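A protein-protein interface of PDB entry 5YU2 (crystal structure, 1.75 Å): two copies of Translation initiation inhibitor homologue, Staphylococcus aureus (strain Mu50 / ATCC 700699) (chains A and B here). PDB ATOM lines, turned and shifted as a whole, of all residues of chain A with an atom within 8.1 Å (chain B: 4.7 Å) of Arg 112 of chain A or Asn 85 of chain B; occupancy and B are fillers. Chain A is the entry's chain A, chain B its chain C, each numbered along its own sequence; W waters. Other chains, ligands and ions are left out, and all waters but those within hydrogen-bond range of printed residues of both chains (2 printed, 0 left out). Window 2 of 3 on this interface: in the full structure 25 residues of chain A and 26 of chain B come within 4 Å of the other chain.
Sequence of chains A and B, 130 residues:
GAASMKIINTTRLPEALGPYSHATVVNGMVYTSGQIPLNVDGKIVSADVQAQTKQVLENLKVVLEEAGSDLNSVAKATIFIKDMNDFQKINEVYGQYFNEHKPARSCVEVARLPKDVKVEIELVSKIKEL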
ATOM      1  N   PHE A  80       3.646 -27.323 -10.905  1.00  0.00           N
ATOM      2  CA  PHE A  80       3.753 -27.328 -12.332  1.00  0.00           C
ATOM      3  C   PHE A  80       4.603 -28.500 -12.780  1.00  0.00           C
ATOM      4  O   PHE A  80       5.711 -28.750 -12.256  1.00  0.00           O
ATOM      5  CB  PHE A  80       4.442 -26.015 -12.777  1.00  0.00           C
ATOM      6  CG  PHE A  80       3.774 -24.753 -12.365  1.00  0.00           C
ATOM      7  CD1 PHE A  80       2.636 -24.335 -12.976  1.00  0.00           C
ATOM      8  CD2 PHE A  80       4.351 -23.929 -11.395  1.00  0.00           C
ATOM      9  CE1 PHE A  80       2.030 -23.115 -12.671  1.00  0.00           C
ATOM     10  CE2 PHE A  80       3.721 -22.741 -11.060  1.00  0.00           C
ATOM     11  CZ  PHE A  80       2.554 -22.357 -11.721  1.00  0.00           C
ATOM     12  N   ILE A  81       4.127 -29.264 -13.773  1.00  0.00           N
ATOM     13  CA  ILE A  81       4.776 -30.460 -14.157  1.00  0.00           C
ATOM     14  C   ILE A  81       4.931 -30.536 -15.644  1.00  0.00           C
ATOM     15  O   ILE A  81       4.159 -29.898 -16.416  1.00  0.00           O
ATOM     16  CB  ILE A  81       4.086 -31.762 -13.642  1.00  0.00           C
ATOM     17  CG1 ILE A  81       2.743 -32.007 -14.222  1.00  0.00           C
ATOM     18  CG2 ILE A  81       3.959 -31.665 -12.133  1.00  0.00           C
ATOM     19  CD1 ILE A  81       2.200 -33.368 -13.805  1.00  0.00           C
ATOM     20  N   LYS A  82       5.945 -31.315 -16.045  1.00  0.00           N
ATOM     21  CA  LYS A  82       6.164 -31.519 -17.496  1.00  0.00           C
ATOM     22  C   LYS A  82       5.304 -32.580 -18.089  1.00  0.00           C
ATOM     23  O   LYS A  82       4.988 -32.546 -19.287  1.00  0.00           O
ATOM     24  CB  LYS A  82       7.652 -31.725 -17.812  1.00  0.00           C
ATOM     25  CG  LYS A  82       7.979 -32.031 -19.326  1.00  0.00           C
ATOM     26  CD  LYS A  82       7.555 -30.880 -20.267  1.00  0.00           C
ATOM     27  CE  LYS A  82       7.578 -31.296 -21.761  1.00  0.00           C
ATOM     28  NZ  LYS A  82       6.418 -32.120 -22.055  1.00  0.00           N
ATOM     29  N   GLU A 109      -0.088 -29.482 -16.110  1.00  0.00           N
ATOM     30  CA  GLU A 109       1.025 -29.795 -17.065  1.00  0.00           C
ATOM     31  C   GLU A 109       1.284 -28.592 -17.891  1.00  0.00           C
ATOM     32  O   GLU A 109       0.396 -28.121 -18.590  1.00  0.00           O
ATOM     33  CB  GLU A 109       0.797 -31.026 -17.885  1.00  0.00           C
ATOM     34  CG  GLU A 109       2.018 -31.446 -18.683  1.00  0.00           C
ATOM     35  CD  GLU A 109       1.712 -32.514 -19.702  1.00  0.00           C
ATOM     36  OE1 GLU A 109       2.009 -32.259 -20.906  1.00  0.00           O
ATOM     37  OE2 GLU A 109       1.240 -33.635 -19.307  1.00  0.00           O
ATOM     38  N   VAL A 110       2.512 -28.101 -17.776  1.00  0.00           N
ATOM     39  CA  VAL A 110       2.948 -26.926 -18.563  1.00  0.00           C
ATOM     40  C   VAL A 110       3.699 -27.452 -19.790  1.00  0.00           C
ATOM     41  O   VAL A 110       3.984 -28.611 -19.912  1.00  0.00           O
ATOM     42  CB  VAL A 110       3.774 -25.933 -17.742  1.00  0.00           C
ATOM     43  CG1 VAL A 110       2.975 -25.437 -16.547  1.00  0.00           C
ATOM     44  CG2 VAL A 110       5.056 -26.521 -17.263  1.00  0.00           C
ATOM     45  N   ALA A 111       3.973 -26.555 -20.706  1.00  0.00           N
ATOM     46  CA  ALA A 111       4.712 -26.933 -21.936  1.00  0.00           C
ATOM     47  C   ALA A 111       6.201 -27.144 -21.630  1.00  0.00           C
ATOM     48  O   ALA A 111       6.854 -28.024 -22.221  1.00  0.00           O
ATOM     49  CB  ALA A 111       4.536 -25.813 -22.941  1.00  0.00           C
ATOM     50  N   ARG A 112       6.774 -26.361 -20.738  1.00  0.00           N
ATOM     51  CA  ARG A 112       8.196 -26.430 -20.411  1.00  0.00           C
ATOM     52  C   ARG A 112       8.499 -25.680 -19.126  1.00  0.00           C
ATOM     53  O   ARG A 112       7.874 -24.654 -18.871  1.00  0.00           O
ATOM     54  CB  ARG A 112       9.038 -25.841 -21.610  1.00  0.00           C
ATOM     55  CG  ARG A 112      10.457 -26.363 -21.645  1.00  0.00           C
ATOM     56  CD  ARG A 112      11.135 -25.779 -22.887  1.00  0.00           C
ATOM     57  NE  ARG A 112      12.557 -26.179 -22.907  1.00  0.00           N
ATOM     58  CZ  ARG A 112      13.516 -25.538 -23.577  1.00  0.00           C
ATOM     59  NH1 ARG A 112      13.253 -24.436 -24.296  1.00  0.00           N
ATOM     60  NH2 ARG A 112      14.787 -25.997 -23.516  1.00  0.00           N
ATOM     61  N   LEU A 113       9.461 -26.202 -18.380  1.00  0.00           N
ATOM     62  CA  LEU A 113       9.959 -25.666 -17.134  1.00  0.00           C
ATOM     63  C   LEU A 113      11.382 -25.197 -17.323  1.00  0.00           C
ATOM     64  O   LEU A 113      12.086 -25.691 -18.248  1.00  0.00           O
ATOM     65  CB  LEU A 113       9.819 -26.667 -15.942  1.00  0.00           C
ATOM     66  CG  LEU A 113       8.372 -26.994 -15.530  1.00  0.00           C
ATOM     67  CD1 LEU A 113       8.402 -28.209 -14.611  1.00  0.00           C
ATOM     68  CD2 LEU A 113       7.698 -25.781 -14.938  1.00  0.00           C
ATOM     69  N   PRO A 114      11.840 -24.331 -16.428  1.00  0.00           N
ATOM     70  CA  PRO A 114      13.211 -23.867 -16.422  1.00  0.00           C
ATOM     71  C   PRO A 114      14.186 -25.024 -16.443  1.00  0.00           C
ATOM     72  O   PRO A 114      13.981 -26.019 -15.745  1.00  0.00           O
ATOM     73  CB  PRO A 114      13.319 -23.131 -15.116  1.00  0.00           C
ATOM     74  CG  PRO A 114      11.966 -22.497 -14.916  1.00  0.00           C
ATOM     75  CD  PRO A 114      11.087 -23.641 -15.348  1.00  0.00           C
ATOM     76  N   LYS A 115      15.197 -24.954 -17.328  1.00  0.00           N
ATOM     77  CA  LYS A 115      16.184 -25.995 -17.349  1.00  0.00           C
ATOM     78  C   LYS A 115      15.654 -27.407 -17.750  1.00  0.00           C
ATOM     79  O   LYS A 115      16.315 -28.425 -17.534  1.00  0.00           O
ATOM     80  CB  LYS A 115      17.019 -25.980 -16.067  1.00  0.00           C
ATOM     81  CG  LYS A 115      17.632 -24.665 -15.682  1.00  0.00           C
ATOM     82  CD  LYS A 115      18.540 -24.909 -14.472  1.00  0.00           C
ATOM     83  CE  LYS A 115      18.995 -23.691 -13.766  1.00  0.00           C
ATOM     84  NZ  LYS A 115      19.843 -22.899 -14.669  1.00  0.00           N
ATOM     85  N   ASP A 116      14.460 -27.493 -18.375  1.00  0.00           N
ATOM     86  CA  ASP A 116      13.884 -28.737 -18.708  1.00  0.00           C
ATOM     87  C   ASP A 116      13.667 -29.719 -17.527  1.00  0.00           C
ATOM     88  O   ASP A 116      13.661 -30.929 -17.670  1.00  0.00           O
ATOM     89  CB  ASP A 116      14.633 -29.394 -19.859  1.00  0.00           C
ATOM     90  CG  ASP A 116      14.431 -28.653 -21.119  1.00  0.00           C
ATOM     91  OD1 ASP A 116      13.280 -28.565 -21.658  1.00  0.00           O
ATOM     92  OD2 ASP A 116      15.418 -28.102 -21.611  1.00  0.00           O
ATOM     93  N   VAL A 117      13.441 -29.144 -16.361  1.00  0.00           N
ATOM     94  CA  VAL A 117      13.161 -29.976 -15.190  1.00  0.00           C
ATOM     95  C   VAL A 117      11.725 -30.569 -15.335  1.00  0.00           C
ATOM     96  O   VAL A 117      10.966 -30.162 -16.150  1.00  0.00           O
ATOM     97  CB  VAL A 117      13.298 -29.235 -13.848  1.00  0.00           C
ATOM     98  CG1 VAL A 117      14.742 -28.685 -13.654  1.00  0.00           C
ATOM     99  CG2 VAL A 117      12.277 -28.094 -13.683  1.00  0.00           C
ATOM    100  N   LYS A 118      11.384 -31.508 -14.488  1.00  0.00           N
ATOM    101  CA  LYS A 118      10.106 -32.190 -14.594  1.00  0.00           C
ATOM    102  C   LYS A 118       9.064 -31.697 -13.629  1.00  0.00           C
ATOM    103  O   LYS A 118       7.903 -32.029 -13.824  1.00  0.00           O
ATOM    104  CB  LYS A 118      10.314 -33.711 -14.403  1.00  0.00           C
ATOM    105  CG  LYS A 118      11.248 -34.308 -15.512  1.00  0.00           C
ATOM    106  CD  LYS A 118      11.608 -35.739 -15.115  1.00  0.00           C
ATOM    107  CE  LYS A 118      12.174 -36.543 -16.274  1.00  0.00           C
ATOM    108  NZ  LYS A 118      13.645 -36.291 -16.326  1.00  0.00           N
ATOM    109  N   GLU A 120       8.114 -28.280 -10.704  1.00  0.00           N
ATOM    110  CA  GLU A 120       8.387 -27.041 -10.025  1.00  0.00           C
ATOM    111  C   GLU A 120       7.231 -26.726  -9.100  1.00  0.00           C
ATOM    112  O   GLU A 120       6.046 -26.878  -9.524  1.00  0.00           O
ATOM    113  CB  GLU A 120       8.565 -25.930 -11.051  1.00  0.00           C
ATOM    114  CG  GLU A 120       8.708 -24.546 -10.423  1.00  0.00           C
ATOM    115  CD  GLU A 120       9.175 -23.479 -11.348  1.00  0.00           C
ATOM    116  OE1 GLU A 120       9.329 -23.673 -12.566  1.00  0.00           O
ATOM    117  OE2 GLU A 120       9.318 -22.382 -10.813  1.00  0.00           O
ATOM    118  N   ASP B  83       7.511 -19.073 -24.831  1.00  0.00           N
ATOM    119  CA  ASP B  83       8.755 -19.758 -25.145  1.00  0.00           C
ATOM    120  C   ASP B  83       9.838 -19.532 -24.100  1.00  0.00           C
ATOM    121  O   ASP B  83      10.193 -18.399 -23.776  1.00  0.00           O
ATOM    122  CB  ASP B  83       9.264 -19.330 -26.524  1.00  0.00           C
ATOM    123  CG  ASP B  83      10.284 -20.297 -27.095  1.00  0.00           C
ATOM    124  OD1 ASP B  83      10.859 -21.085 -26.315  1.00  0.00           O
ATOM    125  OD2 ASP B  83      10.510 -20.267 -28.322  1.00  0.00           O
ATOM    126  N   MET B  84      10.340 -20.645 -23.575  1.00  0.00           N
ATOM    127  CA  MET B  84      11.388 -20.627 -22.573  1.00  0.00           C
ATOM    128  C   MET B  84      12.675 -20.125 -23.205  1.00  0.00           C
ATOM    129  O   MET B  84      13.502 -19.511 -22.531  1.00  0.00           O
ATOM    130  CB  MET B  84      11.598 -22.025 -21.989  1.00  0.00           C
ATOM    131  CG  MET B  84      12.282 -22.035 -20.632  1.00  0.00           C
ATOM    132  SD  MET B  84      11.607 -20.802 -19.503  1.00  0.00           S
ATOM    133  CE  MET B  84      10.297 -21.738 -18.722  1.00  0.00           C
ATOM    134  N   ASN B  85      12.849 -20.381 -24.499  1.00  0.00           N
ATOM    135  CA  ASN B  85      14.106 -19.895 -25.184  1.00  0.00           C
ATOM    136  C   ASN B  85      14.165 -18.378 -25.230  1.00  0.00           C
ATOM    137  O   ASN B  85      15.285 -17.824 -25.389  1.00  0.00           O
ATOM    138  CB  ASN B  85      14.209 -20.548 -26.555  1.00  0.00           C
ATOM    139  CG  ASN B  85      14.484 -22.084 -26.428  1.00  0.00           C
ATOM    140  OD1 ASN B  85      15.197 -22.554 -25.478  1.00  0.00           O
ATOM    141  ND2 ASN B  85      13.878 -22.849 -27.324  1.00  0.00           N
ATOM    142  N   ASP B  86      13.014 -17.695 -24.988  1.00  0.00           N
ATOM    143  CA  ASP B  86      13.025 -16.248 -24.742  1.00  0.00           C
ATOM    144  C   ASP B  86      13.189 -15.798 -23.313  1.00  0.00           C
ATOM    145  O   ASP B  86      13.180 -14.612 -23.111  1.00  0.00           O
ATOM    146  CB  ASP B  86      11.816 -15.602 -25.406  1.00  0.00           C
ATOM    147  CG  ASP B  86      11.936 -15.611 -26.934  1.00  0.00           C
ATOM    148  OD1 ASP B  86      13.079 -15.546 -27.441  1.00  0.00           O
ATOM    149  OD2 ASP B  86      10.941 -15.582 -27.596  1.00  0.00           O
ATOM    150  N   PHE B  87      13.367 -16.697 -22.353  1.00  0.00           N
ATOM    151  CA  PHE B  87      13.461 -16.349 -20.988  1.00  0.00           C
ATOM    152  C   PHE B  87      14.496 -15.296 -20.687  1.00  0.00           C
ATOM    153  O   PHE B  87      14.250 -14.363 -19.966  1.00  0.00           O
ATOM    154  CB  PHE B  87      13.706 -17.529 -20.074  1.00  0.00           C
ATOM    155  CG  PHE B  87      13.769 -17.127 -18.651  1.00  0.00           C
ATOM    156  CD1 PHE B  87      12.635 -16.699 -17.998  1.00  0.00           C
ATOM    157  CD2 PHE B  87      15.011 -16.992 -18.008  1.00  0.00           C
ATOM    158  CE1 PHE B  87      12.692 -16.210 -16.685  1.00  0.00           C
ATOM    159  CE2 PHE B  87      15.065 -16.520 -16.715  1.00  0.00           C
ATOM    160  CZ  PHE B  87      13.915 -16.167 -16.054  1.00  0.00           C
ATOM    161  N   VAL B 108       6.887 -20.083 -15.947  1.00  0.00           N
ATOM    162  CA  VAL B 108       6.673 -21.322 -16.678  1.00  0.00           C
ATOM    163  C   VAL B 108       6.281 -21.018 -18.120  1.00  0.00           C
ATOM    164  O   VAL B 108       5.665 -19.990 -18.429  1.00  0.00           O
ATOM    165  CB  VAL B 108       5.609 -22.229 -16.015  1.00  0.00           C
ATOM    166  CG1 VAL B 108       6.045 -22.603 -14.591  1.00  0.00           C
ATOM    167  CG2 VAL B 108       4.203 -21.652 -16.079  1.00  0.00           C
ATOM    168  N   GLU B 109       6.575 -21.970 -19.002  1.00  0.00           N
ATOM    169  CA  GLU B 109       6.151 -21.927 -20.370  1.00  0.00           C
ATOM    170  C   GLU B 109       4.804 -22.618 -20.526  1.00  0.00           C
ATOM    171  O   GLU B 109       4.666 -23.803 -20.212  1.00  0.00           O
ATOM    172  CB  GLU B 109       7.218 -22.525 -21.362  1.00  0.00           C
ATOM    173  CG  GLU B 109       6.763 -22.440 -22.797  1.00  0.00           C
ATOM    174  CD  GLU B 109       7.676 -23.208 -23.801  1.00  0.00           C
ATOM    175  OE1 GLU B 109       7.108 -23.902 -24.691  1.00  0.00           O
ATOM    176  OE2 GLU B 109       8.914 -23.077 -23.687  1.00  0.00           O
HETATM  177  O   HOH W   1      10.732 -23.629 -25.479  1.00  0.00           O
HETATM  178  O   HOH W   2      14.784 -25.572 -27.226  1.00  0.00           O
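Among the printed residues, merely in contact across the chains: Phe 80 of chain A with Val 108 of chain B, Val 110 of chain A with Glu 109 of chain B, Arg 112 of chain A with Met 84 of chain B, Leu 113 of chain A with Met 84 of chain B, Leu 113 of chain A with Val 108 of chain B and Pro 114 of chain A with Met 84 of chain B.
Asn 85 of chain B touches just one residue of chain A: Arg 112 (3.0 Å).
Printed residues of chain B within 4 Å of Pro 114 of chain A: Met 84.
Printed residues of chain B within 4 Å of Phe 80 of chain A: Val 108.
Of the printed residues of chain A, Val 108 of chain B touches Phe 80 and Leu 113.
Asp 86 of chain B touches none of the printed residues of chain A.
Glu 120 of chain A touches none of the printed residues of chain B.
The nearest residue of chain A that does not touch Asn 85 of chain B is Asp 116 of chain A (6.8 Å).
The backbone carbonyl oxygen (O) of Glu 120 of chain A lies within hydrogen-bond range of the backbone NH (N) of Phe 80 of chain A, 2.8 Å away.
The backbone carbonyl oxygen (O) of Ile 81 of chain A is in hydrogen-bond range of the backbone NH (N) of Val 110 of chain A (2.8 Å).
The guanidinium group of Arg 112 of chain A lies within salt-bridge range of the side-chain carboxylate of Asp 116 of chain A, 2.8 Å away.
The side-chain carboxylate (OD1) of Asp 83 of chain B is in hydrogen-bond range of the backbone NH (N) of Asn 85 of chain B (2.8 Å).
N of Met 84 of chain B is in hydrogen-bond range of OE2 of Glu 109 of chain B (2.8 Å).
N of Ala 111 of chain A is in hydrogen-bond range of O of Glu 109 of chain B.
The guanidinium group (NH1) of Arg 112 of chain A lies within hydrogen-bond range of the side-chain amide oxygen (OD1) of Asn 85 of chain B (3.0 Å).
O of Arg 112 of chain A is in hydrogen-bond range of N of Glu 109 of chain B (3.0 Å).
1 position is printed for both chains.
Of the 9 pairs that touch across the chains among the printed residues, none has its exchanged pair printed and touching as well.
Printed residues of chain B that touch a printed residue of chain A: Met 84, Asn 85, Val 108 and Glu 109.
Hydrophobic or aromatic side chains of chain A that line the printed part of chain B: Phe 80, Val 110, Ala 111, Leu 113 and Pro 114.
Among the printed residues, no Asp or Glu carboxylate lies within 4 Å of a Lys or Arg side-chain nitrogen of the other chain.
Water W1 lies within hydrogen-bond range of the side-chain carboxylate (OE2) of Glu 109 of chain B (2.6 Å), the side-chain carboxylate (OD1) of Asp 83 of chain B (2.7 Å) and the guanidinium group (NH1) of Arg 112 of chain A (2.9 Å).
Water W2 bridges ND2 of Asn 85 of chain B (2.9 Å) and NH1 of Arg 112 of chain A (3.5 Å).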
